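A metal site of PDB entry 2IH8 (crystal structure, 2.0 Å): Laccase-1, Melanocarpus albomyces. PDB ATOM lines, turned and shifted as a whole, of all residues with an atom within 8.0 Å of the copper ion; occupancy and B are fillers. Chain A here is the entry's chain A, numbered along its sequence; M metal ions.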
ATOM      1  N   GLU A 235      -0.158 -12.816 -16.232  1.00  0.00           N
ATOM      2  CA  GLU A 235      -1.509 -13.368 -16.002  1.00  0.00           C
ATOM      3  C   GLU A 235      -1.667 -14.853 -16.319  1.00  0.00           C
ATOM      4  O   GLU A 235      -2.333 -15.569 -15.564  1.00  0.00           O
ATOM      5  CB  GLU A 235      -2.564 -12.544 -16.776  1.00  0.00           C
ATOM      6  CG  GLU A 235      -4.062 -12.865 -16.465  1.00  0.00           C
ATOM      7  CD  GLU A 235      -4.631 -14.031 -17.266  1.00  0.00           C
ATOM      8  OE1 GLU A 235      -4.053 -14.389 -18.312  1.00  0.00           O
ATOM      9  OE2 GLU A 235      -5.644 -14.635 -16.838  1.00  0.00           O
ATOM     10  N   HIS A 237      -1.592 -18.764 -16.745  1.00  0.00           N
ATOM     11  CA  HIS A 237      -1.257 -19.933 -15.934  1.00  0.00           C
ATOM     12  C   HIS A 237      -1.156 -21.068 -16.928  1.00  0.00           C
ATOM     13  O   HIS A 237      -2.116 -21.345 -17.664  1.00  0.00           O
ATOM     14  CB  HIS A 237      -2.355 -20.234 -14.940  1.00  0.00           C
ATOM     15  CG  HIS A 237      -2.540 -19.201 -13.885  1.00  0.00           C
ATOM     16  ND1 HIS A 237      -2.800 -17.877 -14.175  1.00  0.00           N
ATOM     17  CD2 HIS A 237      -2.586 -19.305 -12.541  1.00  0.00           C
ATOM     18  CE1 HIS A 237      -2.999 -17.221 -13.047  1.00  0.00           C
ATOM     19  NE2 HIS A 237      -2.875 -18.063 -12.041  1.00  0.00           N
ATOM     20  N   VAL A 361     -11.091 -12.080   0.189  1.00  0.00           N
ATOM     21  CA  VAL A 361     -10.775 -11.442  -1.088  1.00  0.00           C
ATOM     22  C   VAL A 361     -12.139 -11.119  -1.693  1.00  0.00           C
ATOM     23  O   VAL A 361     -13.070 -11.915  -1.577  1.00  0.00           O
ATOM     24  CB  VAL A 361      -9.976 -12.405  -2.027  1.00  0.00           C
ATOM     25  CG1 VAL A 361      -9.820 -11.828  -3.439  1.00  0.00           C
ATOM     26  CG2 VAL A 361      -8.601 -12.666  -1.441  1.00  0.00           C
ATOM     27  N   TRP A 373      -9.960  -4.862  -6.569  1.00  0.00           N
ATOM     28  CA  TRP A 373      -9.820  -6.043  -5.708  1.00  0.00           C
ATOM     29  C   TRP A 373      -9.506  -5.652  -4.285  1.00  0.00           C
ATOM     30  O   TRP A 373      -8.515  -4.968  -4.029  1.00  0.00           O
ATOM     31  CB  TRP A 373      -8.732  -6.957  -6.260  1.00  0.00           C
ATOM     32  CG  TRP A 373      -9.094  -7.596  -7.563  1.00  0.00           C
ATOM     33  CD1 TRP A 373      -8.749  -7.163  -8.813  1.00  0.00           C
ATOM     34  CD2 TRP A 373      -9.908  -8.764  -7.752  1.00  0.00           C
ATOM     35  NE1 TRP A 373      -9.290  -7.976  -9.772  1.00  0.00           N
ATOM     36  CE2 TRP A 373     -10.008  -8.979  -9.156  1.00  0.00           C
ATOM     37  CE3 TRP A 373     -10.563  -9.654  -6.879  1.00  0.00           C
ATOM     38  CZ2 TRP A 373     -10.746 -10.039  -9.714  1.00  0.00           C
ATOM     39  CZ3 TRP A 373     -11.309 -10.729  -7.438  1.00  0.00           C
ATOM     40  CH2 TRP A 373     -11.393 -10.900  -8.843  1.00  0.00           C
ATOM     41  N   ASN A 421     -12.078 -16.792  -1.229  1.00  0.00           N
ATOM     42  CA  ASN A 421     -12.202 -16.232  -2.580  1.00  0.00           C
ATOM     43  C   ASN A 421     -13.592 -15.755  -2.989  1.00  0.00           C
ATOM     44  O   ASN A 421     -14.290 -16.458  -3.749  1.00  0.00           O
ATOM     45  CB  ASN A 421     -11.690 -17.232  -3.615  1.00  0.00           C
ATOM     46  CG  ASN A 421     -11.279 -16.573  -4.928  1.00  0.00           C
ATOM     47  OD1 ASN A 421     -11.482 -15.373  -5.136  1.00  0.00           O
ATOM     48  ND2 ASN A 421     -10.685 -17.363  -5.811  1.00  0.00           N
ATOM     49  N   LEU A 429     -12.775 -15.786  -9.575  1.00  0.00           N
ATOM     50  CA  LEU A 429     -11.692 -16.245 -10.423  1.00  0.00           C
ATOM     51  C   LEU A 429     -10.580 -16.852  -9.581  1.00  0.00           C
ATOM     52  O   LEU A 429     -10.434 -16.487  -8.415  1.00  0.00           O
ATOM     53  CB  LEU A 429     -11.106 -15.043 -11.192  1.00  0.00           C
ATOM     54  CG  LEU A 429     -11.978 -14.176 -12.089  1.00  0.00           C
ATOM     55  CD1 LEU A 429     -11.155 -12.981 -12.570  1.00  0.00           C
ATOM     56  CD2 LEU A 429     -12.514 -14.969 -13.276  1.00  0.00           C
ATOM     57  N   PRO A 430      -9.789 -17.802 -10.144  1.00  0.00           N
ATOM     58  CA  PRO A 430      -8.695 -18.402  -9.380  1.00  0.00           C
ATOM     59  C   PRO A 430      -7.587 -17.347  -9.194  1.00  0.00           C
ATOM     60  O   PRO A 430      -7.454 -16.442 -10.036  1.00  0.00           O
ATOM     61  CB  PRO A 430      -8.209 -19.513 -10.310  1.00  0.00           C
ATOM     62  CG  PRO A 430      -9.418 -19.858 -11.096  1.00  0.00           C
ATOM     63  CD  PRO A 430      -9.972 -18.525 -11.415  1.00  0.00           C
ATOM     64  N   HIS A 431      -6.885 -17.395  -8.071  1.00  0.00           N
ATOM     65  CA  HIS A 431      -5.820 -16.436  -7.776  1.00  0.00           C
ATOM     66  C   HIS A 431      -4.513 -17.083  -7.312  1.00  0.00           C
ATOM     67  O   HIS A 431      -4.525 -17.852  -6.353  1.00  0.00           O
ATOM     68  CB  HIS A 431      -6.236 -15.421  -6.690  1.00  0.00           C
ATOM     69  CG  HIS A 431      -7.392 -14.546  -7.076  1.00  0.00           C
ATOM     70  ND1 HIS A 431      -7.285 -13.553  -8.022  1.00  0.00           N
ATOM     71  CD2 HIS A 431      -8.684 -14.557  -6.685  1.00  0.00           C
ATOM     72  CE1 HIS A 431      -8.471 -12.988  -8.195  1.00  0.00           C
ATOM     73  NE2 HIS A 431      -9.328 -13.592  -7.394  1.00  0.00           N
ATOM     74  N   PRO A 432      -3.395 -16.813  -8.012  1.00  0.00           N
ATOM     75  CA  PRO A 432      -2.095 -17.378  -7.623  1.00  0.00           C
ATOM     76  C   PRO A 432      -1.528 -16.533  -6.465  1.00  0.00           C
ATOM     77  O   PRO A 432      -0.953 -15.469  -6.679  1.00  0.00           O
ATOM     78  CB  PRO A 432      -1.265 -17.252  -8.901  1.00  0.00           C
ATOM     79  CG  PRO A 432      -1.825 -16.038  -9.559  1.00  0.00           C
ATOM     80  CD  PRO A 432      -3.309 -16.213  -9.361  1.00  0.00           C
ATOM     81  N   MET A 433      -1.770 -17.002  -5.247  1.00  0.00           N
ATOM     82  CA  MET A 433      -1.320 -16.287  -4.047  1.00  0.00           C
ATOM     83  C   MET A 433       0.154 -16.511  -3.764  1.00  0.00           C
ATOM     84  O   MET A 433       0.617 -17.651  -3.673  1.00  0.00           O
ATOM     85  CB  MET A 433      -2.183 -16.662  -2.850  1.00  0.00           C
ATOM     86  CG  MET A 433      -3.658 -16.332  -3.011  1.00  0.00           C
ATOM     87  SD  MET A 433      -4.026 -14.627  -3.511  1.00  0.00           S
ATOM     88  CE  MET A 433      -3.606 -13.715  -2.011  1.00  0.00           C
ATOM     89  N   MET A 480      -2.350 -21.843  -5.607  1.00  0.00           N
ATOM     90  CA  MET A 480      -3.648 -21.381  -6.077  1.00  0.00           C
ATOM     91  C   MET A 480      -4.761 -21.276  -5.046  1.00  0.00           C
ATOM     92  O   MET A 480      -4.958 -22.164  -4.219  1.00  0.00           O
ATOM     93  CB  MET A 480      -4.148 -22.250  -7.223  1.00  0.00           C
ATOM     94  CG  MET A 480      -3.278 -22.223  -8.461  1.00  0.00           C
ATOM     95  SD  MET A 480      -3.036 -20.574  -9.124  1.00  0.00           S
ATOM     96  CE  MET A 480      -4.659 -20.159  -9.699  1.00  0.00           C
ATOM     97  N   LEU A 481      -5.463 -20.142  -5.114  1.00  0.00           N
ATOM     98  CA  LEU A 481      -6.630 -19.887  -4.285  1.00  0.00           C
ATOM     99  C   LEU A 481      -7.743 -20.293  -5.276  1.00  0.00           C
ATOM    100  O   LEU A 481      -7.894 -19.659  -6.319  1.00  0.00           O
ATOM    101  CB  LEU A 481      -6.727 -18.392  -3.942  1.00  0.00           C
ATOM    102  CG  LEU A 481      -7.983 -17.822  -3.296  1.00  0.00           C
ATOM    103  CD1 LEU A 481      -8.278 -18.448  -1.952  1.00  0.00           C
ATOM    104  CD2 LEU A 481      -7.865 -16.321  -3.165  1.00  0.00           C
ATOM    105  N   HIS A 502       0.309 -11.370  -1.897  1.00  0.00           N
ATOM    106  CA  HIS A 502      -0.536 -10.944  -2.991  1.00  0.00           C
ATOM    107  C   HIS A 502      -0.794 -11.941  -4.083  1.00  0.00           C
ATOM    108  O   HIS A 502      -0.091 -12.944  -4.207  1.00  0.00           O
ATOM    109  CB  HIS A 502       0.060  -9.684  -3.626  1.00  0.00           C
ATOM    110  CG  HIS A 502       1.425  -9.874  -4.224  1.00  0.00           C
ATOM    111  ND1 HIS A 502       1.615 -10.118  -5.563  1.00  0.00           N
ATOM    112  CD2 HIS A 502       2.666  -9.817  -3.671  1.00  0.00           C
ATOM    113  CE1 HIS A 502       2.917 -10.195  -5.818  1.00  0.00           C
ATOM    114  NE2 HIS A 502       3.569 -10.016  -4.689  1.00  0.00           N
ATOM    115  N   CYS A 503      -1.782 -11.617  -4.924  1.00  0.00           N
ATOM    116  CA  CYS A 503      -2.083 -12.412  -6.101  1.00  0.00           C
ATOM    117  C   CYS A 503      -1.011 -11.970  -7.088  1.00  0.00           C
ATOM    118  O   CYS A 503      -0.733 -10.777  -7.212  1.00  0.00           O
ATOM    119  CB  CYS A 503      -3.454 -12.069  -6.657  1.00  0.00           C
ATOM    120  SG  CYS A 503      -3.695 -12.843  -8.256  1.00  0.00           S
ATOM    121  N   HIS A 504      -0.402 -12.935  -7.777  1.00  0.00           N
ATOM    122  CA  HIS A 504       0.647 -12.603  -8.731  1.00  0.00           C
ATOM    123  C   HIS A 504       0.171 -12.206 -10.125  1.00  0.00           C
ATOM    124  O   HIS A 504       0.994 -11.923 -11.004  1.00  0.00           O
ATOM    125  CB  HIS A 504       1.715 -13.677  -8.787  1.00  0.00           C
ATOM    126  CG  HIS A 504       3.101 -13.126  -8.913  1.00  0.00           C
ATOM    127  ND1 HIS A 504       3.547 -12.492 -10.048  1.00  0.00           N
ATOM    128  CD2 HIS A 504       4.123 -13.087  -8.029  1.00  0.00           C
ATOM    129  CE1 HIS A 504       4.790 -12.086  -9.860  1.00  0.00           C
ATOM    130  NE2 HIS A 504       5.170 -12.437  -8.642  1.00  0.00           N
ATOM    131  N   ILE A 505      -1.154 -12.186 -10.328  1.00  0.00           N
ATOM    132  CA  ILE A 505      -1.691 -11.715 -11.608  1.00  0.00           C
ATOM    133  C   ILE A 505      -1.500 -10.202 -11.488  1.00  0.00           C
ATOM    134  O   ILE A 505      -2.043  -9.577 -10.566  1.00  0.00           O
ATOM    135  CB  ILE A 505      -3.190 -12.074 -11.822  1.00  0.00           C
ATOM    136  CG1 ILE A 505      -3.319 -13.563 -12.129  1.00  0.00           C
ATOM    137  CG2 ILE A 505      -3.793 -11.254 -12.995  1.00  0.00           C
ATOM    138  CD1 ILE A 505      -4.760 -14.092 -12.165  1.00  0.00           C
ATOM    139  N   ALA A 506      -0.652  -9.661 -12.362  1.00  0.00           N
ATOM    140  CA  ALA A 506      -0.306  -8.241 -12.380  1.00  0.00           C
ATOM    141  C   ALA A 506      -1.491  -7.300 -12.299  1.00  0.00           C
ATOM    142  O   ALA A 506      -1.514  -6.398 -11.468  1.00  0.00           O
ATOM    143  CB  ALA A 506       0.547  -7.913 -13.588  1.00  0.00           C
ATOM    144  N   TRP A 507      -2.536  -7.614 -13.058  1.00  0.00           N
ATOM    145  CA  TRP A 507      -3.764  -6.827 -13.111  1.00  0.00           C
ATOM    146  C   TRP A 507      -4.517  -6.800 -11.787  1.00  0.00           C
ATOM    147  O   TRP A 507      -5.113  -5.780 -11.440  1.00  0.00           O
ATOM    148  CB  TRP A 507      -4.679  -7.337 -14.229  1.00  0.00           C
ATOM    149  CG  TRP A 507      -4.023  -7.903 -15.511  1.00  0.00           C
ATOM    150  CD1 TRP A 507      -4.438  -9.019 -16.186  1.00  0.00           C
ATOM    151  CD2 TRP A 507      -2.854  -7.430 -16.216  1.00  0.00           C
ATOM    152  NE1 TRP A 507      -3.614  -9.276 -17.252  1.00  0.00           N
ATOM    153  CE2 TRP A 507      -2.628  -8.323 -17.301  1.00  0.00           C
ATOM    154  CE3 TRP A 507      -1.964  -6.344 -16.038  1.00  0.00           C
ATOM    155  CZ2 TRP A 507      -1.546  -8.172 -18.199  1.00  0.00           C
ATOM    156  CZ3 TRP A 507      -0.873  -6.192 -16.931  1.00  0.00           C
ATOM    157  CH2 TRP A 507      -0.688  -7.110 -17.999  1.00  0.00           C
ATOM    158  N   HIS A 508      -4.421  -7.895 -11.041  1.00  0.00           N
ATOM    159  CA  HIS A 508      -5.081  -8.006  -9.745  1.00  0.00           C
ATOM    160  C   HIS A 508      -4.339  -7.299  -8.618  1.00  0.00           C
ATOM    161  O   HIS A 508      -4.979  -6.638  -7.803  1.00  0.00           O
ATOM    162  CB  HIS A 508      -5.349  -9.481  -9.385  1.00  0.00           C
ATOM    163  CG  HIS A 508      -6.293 -10.172 -10.330  1.00  0.00           C
ATOM    164  ND1 HIS A 508      -6.539 -11.526 -10.263  1.00  0.00           N
ATOM    165  CD2 HIS A 508      -6.991  -9.712 -11.391  1.00  0.00           C
ATOM    166  CE1 HIS A 508      -7.362 -11.865 -11.239  1.00  0.00           C
ATOM    167  NE2 HIS A 508      -7.653 -10.782 -11.936  1.00  0.00           N
ATOM    168  N   VAL A 509      -3.010  -7.424  -8.586  1.00  0.00           N
ATOM    169  CA  VAL A 509      -2.204  -6.754  -7.547  1.00  0.00           C
ATOM    170  C   VAL A 509      -2.187  -5.243  -7.810  1.00  0.00           C
ATOM    171  O   VAL A 509      -2.183  -4.443  -6.871  1.00  0.00           O
ATOM    172  CB  VAL A 509      -0.763  -7.371  -7.365  1.00  0.00           C
ATOM    173  CG1 VAL A 509       0.109  -7.198  -8.606  1.00  0.00           C
ATOM    174  CG2 VAL A 509      -0.097  -6.788  -6.124  1.00  0.00           C
ATOM    175  N   LEU A 513      -5.224  -6.357  -4.927  1.00  0.00           N
ATOM    176  CA  LEU A 513      -5.242  -7.656  -4.252  1.00  0.00           C
ATOM    177  C   LEU A 513      -3.929  -7.990  -3.548  1.00  0.00           C
ATOM    178  O   LEU A 513      -3.088  -8.723  -4.097  1.00  0.00           O
ATOM    179  CB  LEU A 513      -5.615  -8.790  -5.216  1.00  0.00           C
ATOM    180  CG  LEU A 513      -6.510  -9.908  -4.663  1.00  0.00           C
ATOM    181  CD1 LEU A 513      -7.008 -10.731  -5.829  1.00  0.00           C
ATOM    182  CD2 LEU A 513      -5.823 -10.818  -3.643  1.00  0.00           C
HETATM  183 CU    CU M   1      -5.789 -12.568  -8.806  1.00  0.00          CU
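The copper ion is bound by ND1 of His 508 (1.9 Å), ND1 of His 431 (2.0 Å) and SG of Cys 503 (2.2 Å).
Ile 505 touches the copper ion. CD1 of Leu 513 touches the copper ion, at 3.7 Å. Of the 21 residues printed, 5 come within 4 Å of the copper ion. Along chain A the residues within 4 Å of the copper ion span positions 431 to 513. The nearest printed residue that does not touch the copper ion is Pro 430 (4.4 Å).
O of His 431 sits at hydrogen-bond distance from N of Leu 481 (2.8 Å). A ring nitrogen (NE2) of His 431 lies close to the backbone carbonyl oxygen (O) of Leu 429 (3.3 Å). N of Ile 505 lies close to SG of Cys 503, 3.3 Å away. The backbone NH (N) of Cys 503 lies within hydrogen-bond range of the backbone carbonyl oxygen (O) of Leu 513 (3.3 Å). O of His 508 is in hydrogen-bond range of N of Leu 513 (2.9 Å).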
